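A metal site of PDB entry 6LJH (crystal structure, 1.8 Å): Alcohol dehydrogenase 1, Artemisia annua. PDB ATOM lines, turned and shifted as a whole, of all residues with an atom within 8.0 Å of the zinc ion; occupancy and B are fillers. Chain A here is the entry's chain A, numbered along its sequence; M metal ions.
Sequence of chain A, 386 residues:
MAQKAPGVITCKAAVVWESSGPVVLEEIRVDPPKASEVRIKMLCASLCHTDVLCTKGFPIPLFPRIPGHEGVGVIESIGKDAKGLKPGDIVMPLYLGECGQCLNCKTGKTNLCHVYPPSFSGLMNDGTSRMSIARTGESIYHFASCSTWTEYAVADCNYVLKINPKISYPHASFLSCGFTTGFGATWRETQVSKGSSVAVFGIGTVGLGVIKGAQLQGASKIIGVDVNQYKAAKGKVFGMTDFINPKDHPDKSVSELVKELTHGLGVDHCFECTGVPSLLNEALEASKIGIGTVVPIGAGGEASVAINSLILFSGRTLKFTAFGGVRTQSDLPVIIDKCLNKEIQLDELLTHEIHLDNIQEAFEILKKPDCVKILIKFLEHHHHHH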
ATOM      1  N   GLY A  97       1.321 -24.573  18.648  1.00  0.00           N
ATOM      2  CA  GLY A  97       0.330 -25.189  17.804  1.00  0.00           C
ATOM      3  C   GLY A  97      -0.631 -24.176  17.229  1.00  0.00           C
ATOM      4  O   GLY A  97      -0.464 -22.959  17.360  1.00  0.00           O
ATOM      5  N   GLU A  98      -1.664 -24.695  16.565  1.00  0.00           N
ATOM      6  CA  GLU A  98      -2.707 -23.833  16.002  1.00  0.00           C
ATOM      7  C   GLU A  98      -4.010 -24.624  16.106  1.00  0.00           C
ATOM      8  O   GLU A  98      -4.239 -25.557  15.325  1.00  0.00           O
ATOM      9  CB  GLU A  98      -2.396 -23.455  14.564  1.00  0.00           C
ATOM     10  CG  GLU A  98      -3.483 -22.587  13.945  1.00  0.00           C
ATOM     11  CD  GLU A  98      -3.224 -22.283  12.481  1.00  0.00           C
ATOM     12  OE1 GLU A  98      -4.121 -21.742  11.818  1.00  0.00           O
ATOM     13  OE2 GLU A  98      -2.102 -22.568  11.996  1.00  0.00           O
ATOM     14  N   CYS A  99      -4.857 -24.259  17.054  1.00  0.00           N
ATOM     15  CA  CYS A  99      -6.105 -24.996  17.251  1.00  0.00           C
ATOM     16  C   CYS A  99      -7.181 -24.563  16.271  1.00  0.00           C
ATOM     17  O   CYS A  99      -8.104 -25.346  16.017  1.00  0.00           O
ATOM     18  CB  CYS A  99      -6.597 -24.839  18.702  1.00  0.00           C
ATOM     19  SG  CYS A  99      -7.497 -23.263  19.080  1.00  0.00           S
ATOM     20  N   GLY A 100      -7.087 -23.354  15.715  1.00  0.00           N
ATOM     21  CA  GLY A 100      -8.045 -22.867  14.742  1.00  0.00           C
ATOM     22  C   GLY A 100      -9.383 -22.424  15.303  1.00  0.00           C
ATOM     23  O   GLY A 100     -10.217 -21.913  14.541  1.00  0.00           O
ATOM     24  N   GLN A 101      -9.608 -22.567  16.606  1.00  0.00           N
ATOM     25  CA  GLN A 101     -10.911 -22.330  17.199  1.00  0.00           C
ATOM     26  C   GLN A 101     -10.917 -21.322  18.343  1.00  0.00           C
ATOM     27  O   GLN A 101     -11.999 -20.847  18.700  1.00  0.00           O
ATOM     28  CB  GLN A 101     -11.510 -23.649  17.733  1.00  0.00           C
ATOM     29  CG  GLN A 101     -11.878 -24.669  16.652  1.00  0.00           C
ATOM     30  CD  GLN A 101     -13.013 -24.189  15.737  1.00  0.00           C
ATOM     31  OE1 GLN A 101     -13.933 -23.491  16.178  1.00  0.00           O
ATOM     32  NE2 GLN A 101     -12.937 -24.568  14.468  1.00  0.00           N
ATOM     33  N   CYS A 102      -9.764 -21.011  18.945  1.00  0.00           N
ATOM     34  CA  CYS A 102      -9.724 -20.115  20.086  1.00  0.00           C
ATOM     35  C   CYS A 102      -9.901 -18.662  19.619  1.00  0.00           C
ATOM     36  O   CYS A 102      -9.956 -18.375  18.426  1.00  0.00           O
ATOM     37  CB  CYS A 102      -8.410 -20.270  20.866  1.00  0.00           C
ATOM     38  SG  CYS A 102      -6.940 -19.623  19.973  1.00  0.00           S
ATOM     39  N   LEU A 103      -9.982 -17.753  20.584  1.00  0.00           N
ATOM     40  CA  LEU A 103     -10.211 -16.344  20.239  1.00  0.00           C
ATOM     41  C   LEU A 103      -9.100 -15.801  19.353  1.00  0.00           C
ATOM     42  O   LEU A 103      -9.371 -15.093  18.369  1.00  0.00           O
ATOM     43  CB  LEU A 103     -10.329 -15.501  21.494  1.00  0.00           C
ATOM     44  CG  LEU A 103     -11.584 -15.779  22.307  1.00  0.00           C
ATOM     45  CD1 LEU A 103     -11.449 -15.063  23.628  1.00  0.00           C
ATOM     46  CD2 LEU A 103     -12.825 -15.312  21.547  1.00  0.00           C
ATOM     47  N   ASN A 104      -7.848 -16.141  19.660  1.00  0.00           N
ATOM     48  CA  ASN A 104      -6.751 -15.614  18.843  1.00  0.00           C
ATOM     49  C   ASN A 104      -6.735 -16.233  17.452  1.00  0.00           C
ATOM     50  O   ASN A 104      -6.534 -15.524  16.452  1.00  0.00           O
ATOM     51  CB  ASN A 104      -5.418 -15.828  19.570  1.00  0.00           C
ATOM     52  CG  ASN A 104      -4.961 -14.585  20.335  1.00  0.00           C
ATOM     53  OD1 ASN A 104      -5.711 -13.604  20.419  1.00  0.00           O
ATOM     54  ND2 ASN A 104      -3.750 -14.628  20.881  1.00  0.00           N
ATOM     55  N   CYS A 105      -6.954 -17.552  17.340  1.00  0.00           N
ATOM     56  CA  CYS A 105      -6.948 -18.197  16.030  1.00  0.00           C
ATOM     57  C   CYS A 105      -8.066 -17.654  15.146  1.00  0.00           C
ATOM     58  O   CYS A 105      -7.876 -17.452  13.939  1.00  0.00           O
ATOM     59  CB  CYS A 105      -7.077 -19.721  16.187  1.00  0.00           C
ATOM     60  SG  CYS A 105      -5.533 -20.583  16.734  1.00  0.00           S
ATOM     61  N   LYS A 106      -9.224 -17.385  15.736  1.00  0.00           N
ATOM     62  CA  LYS A 106     -10.351 -16.919  14.926  1.00  0.00           C
ATOM     63  C   LYS A 106     -10.088 -15.546  14.301  1.00  0.00           C
ATOM     64  O   LYS A 106     -10.642 -15.254  13.232  1.00  0.00           O
ATOM     65  CB  LYS A 106     -11.629 -16.912  15.755  1.00  0.00           C
ATOM     66  CG  LYS A 106     -12.129 -18.319  16.096  1.00  0.00           C
ATOM     67  CD  LYS A 106     -13.649 -18.416  16.008  1.00  0.00           C
ATOM     68  CE  LYS A 106     -14.122 -19.854  15.722  1.00  0.00           C
ATOM     69  NZ  LYS A 106     -14.643 -20.553  16.939  1.00  0.00           N
ATOM     70  N   THR A 110      -2.928 -13.505  14.290  1.00  0.00           N
ATOM     71  CA  THR A 110      -1.852 -13.904  15.183  1.00  0.00           C
ATOM     72  C   THR A 110      -1.616 -15.408  15.077  1.00  0.00           C
ATOM     73  O   THR A 110      -2.519 -16.174  14.746  1.00  0.00           O
ATOM     74  CB  THR A 110      -2.162 -13.504  16.628  1.00  0.00           C
ATOM     75  OG1 THR A 110      -1.094 -13.921  17.489  1.00  0.00           O
ATOM     76  CG2 THR A 110      -3.448 -14.150  17.112  1.00  0.00           C
ATOM     77  N   ASN A 111      -0.381 -15.812  15.352  1.00  0.00           N
ATOM     78  CA  ASN A 111      -0.069 -17.226  15.482  1.00  0.00           C
ATOM     79  C   ASN A 111      -0.017 -17.672  16.944  1.00  0.00           C
ATOM     80  O   ASN A 111       0.323 -18.837  17.212  1.00  0.00           O
ATOM     81  CB  ASN A 111       1.257 -17.556  14.781  1.00  0.00           C
ATOM     82  CG  ASN A 111       2.442 -16.779  15.355  1.00  0.00           C
ATOM     83  OD1 ASN A 111       2.265 -15.706  15.910  1.00  0.00           O
ATOM     84  ND2 ASN A 111       3.662 -17.333  15.222  1.00  0.00           N
ATOM     85  N   LEU A 112      -0.381 -16.799  17.890  1.00  0.00           N
ATOM     86  CA  LEU A 112      -0.186 -17.092  19.310  1.00  0.00           C
ATOM     87  C   LEU A 112      -1.463 -17.724  19.854  1.00  0.00           C
ATOM     88  O   LEU A 112      -2.284 -17.099  20.541  1.00  0.00           O
ATOM     89  CB  LEU A 112       0.232 -15.841  20.083  1.00  0.00           C
ATOM     90  CG  LEU A 112       1.541 -15.247  19.569  1.00  0.00           C
ATOM     91  CD1 LEU A 112       1.994 -14.049  20.412  1.00  0.00           C
ATOM     92  CD2 LEU A 112       2.641 -16.306  19.550  1.00  0.00           C
ATOM     93  N   CYS A 113      -1.620 -19.001  19.527  1.00  0.00           N
ATOM     94  CA  CYS A 113      -2.794 -19.769  19.920  1.00  0.00           C
ATOM     95  C   CYS A 113      -2.940 -19.858  21.431  1.00  0.00           C
ATOM     96  O   CYS A 113      -1.973 -20.105  22.162  1.00  0.00           O
ATOM     97  CB  CYS A 113      -2.681 -21.152  19.282  1.00  0.00           C
ATOM     98  SG  CYS A 113      -3.980 -22.317  19.700  1.00  0.00           S
ATOM     99  N   HIS A 114      -4.181 -19.670  21.916  1.00  0.00           N
ATOM    100  CA  HIS A 114      -4.437 -19.802  23.356  1.00  0.00           C
ATOM    101  C   HIS A 114      -4.352 -21.240  23.826  1.00  0.00           C
ATOM    102  O   HIS A 114      -4.034 -21.489  24.988  1.00  0.00           O
ATOM    103  CB  HIS A 114      -5.815 -19.264  23.710  1.00  0.00           C
ATOM    104  CG  HIS A 114      -5.962 -17.780  23.570  1.00  0.00           C
ATOM    105  ND1 HIS A 114      -7.189 -17.166  23.441  1.00  0.00           N
ATOM    106  CD2 HIS A 114      -5.033 -16.794  23.548  1.00  0.00           C
ATOM    107  CE1 HIS A 114      -7.013 -15.865  23.321  1.00  0.00           C
ATOM    108  NE2 HIS A 114      -5.714 -15.610  23.406  1.00  0.00           N
ATOM    109  N   VAL A 115      -4.653 -22.189  22.950  1.00  0.00           N
ATOM    110  CA  VAL A 115      -4.809 -23.572  23.365  1.00  0.00           C
ATOM    111  C   VAL A 115      -3.484 -24.331  23.320  1.00  0.00           C
ATOM    112  O   VAL A 115      -3.217 -25.170  24.198  1.00  0.00           O
ATOM    113  CB  VAL A 115      -5.881 -24.236  22.478  1.00  0.00           C
ATOM    114  CG1 VAL A 115      -6.020 -25.744  22.781  1.00  0.00           C
ATOM    115  CG2 VAL A 115      -7.229 -23.550  22.676  1.00  0.00           C
ATOM    116  N   TYR A 116      -2.613 -24.024  22.356  1.00  0.00           N
ATOM    117  CA  TYR A 116      -1.313 -24.675  22.185  1.00  0.00           C
ATOM    118  C   TYR A 116      -0.184 -23.653  22.232  1.00  0.00           C
ATOM    119  O   TYR A 116       0.505 -23.421  21.213  1.00  0.00           O
ATOM    120  CB  TYR A 116      -1.283 -25.484  20.885  1.00  0.00           C
ATOM    121  CG  TYR A 116      -2.413 -26.504  20.824  1.00  0.00           C
ATOM    122  CD1 TYR A 116      -2.577 -27.446  21.830  1.00  0.00           C
ATOM    123  CD2 TYR A 116      -3.328 -26.497  19.769  1.00  0.00           C
ATOM    124  CE1 TYR A 116      -3.619 -28.362  21.799  1.00  0.00           C
ATOM    125  CE2 TYR A 116      -4.374 -27.423  19.729  1.00  0.00           C
ATOM    126  CZ  TYR A 116      -4.517 -28.338  20.740  1.00  0.00           C
ATOM    127  OH  TYR A 116      -5.553 -29.251  20.702  1.00  0.00           O
ATOM    128  N   PRO A 117       0.041 -23.021  23.381  1.00  0.00           N
ATOM    129  CA  PRO A 117       1.093 -22.020  23.490  1.00  0.00           C
ATOM    130  C   PRO A 117       2.445 -22.674  23.698  1.00  0.00           C
ATOM    131  O   PRO A 117       2.523 -23.894  23.901  1.00  0.00           O
ATOM    132  CB  PRO A 117       0.669 -21.209  24.720  1.00  0.00           C
ATOM    133  CG  PRO A 117       0.049 -22.241  25.600  1.00  0.00           C
ATOM    134  CD  PRO A 117      -0.689 -23.169  24.664  1.00  0.00           C
HETATM  135 ZN    ZN M   1      -5.973 -21.411  18.854  1.00  0.00          ZN
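The backbone NH (N) of Gly 100 sits close to the side-chain sulfur (SG) of Cys 105. N of His 114 sits close to SG of Cys 102. The side-chain sulfur of Cys 102 sits close to the backbone NH of Asn 104 (3.6 Å). The side-chain sulfur (SG) of Cys 113 sits close to the backbone NH (N) of Val 115 (3.3 Å). The side-chain sulfur (SG) of Cys 113 lies close to the backbone NH (N) of Tyr 116 (3.4 Å). N of Gln 101 sits close to SG of Cys 99 (3.3 Å). NE2 of His 114 lies close to ND2 of Asn 104 (3.3 Å).
Gly 100 touches the zinc ion (N to ZN, 3.9 Å). N of His 114 touches the zinc ion (3.95 Å). Six residues have an atom within 4 Å of the zinc ion: Cys 99, Gly 100, Cys 102, Cys 105, Cys 113 and His 114.
The zinc ion is bound by the side-chain sulfur of Cys 105 (2.3 Å), the side-chain sulfur of Cys 102 (2.3 Å), the side-chain sulfur of Cys 113 (2.3 Å) and the side-chain sulfur of Cys 99 (2.4 Å).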
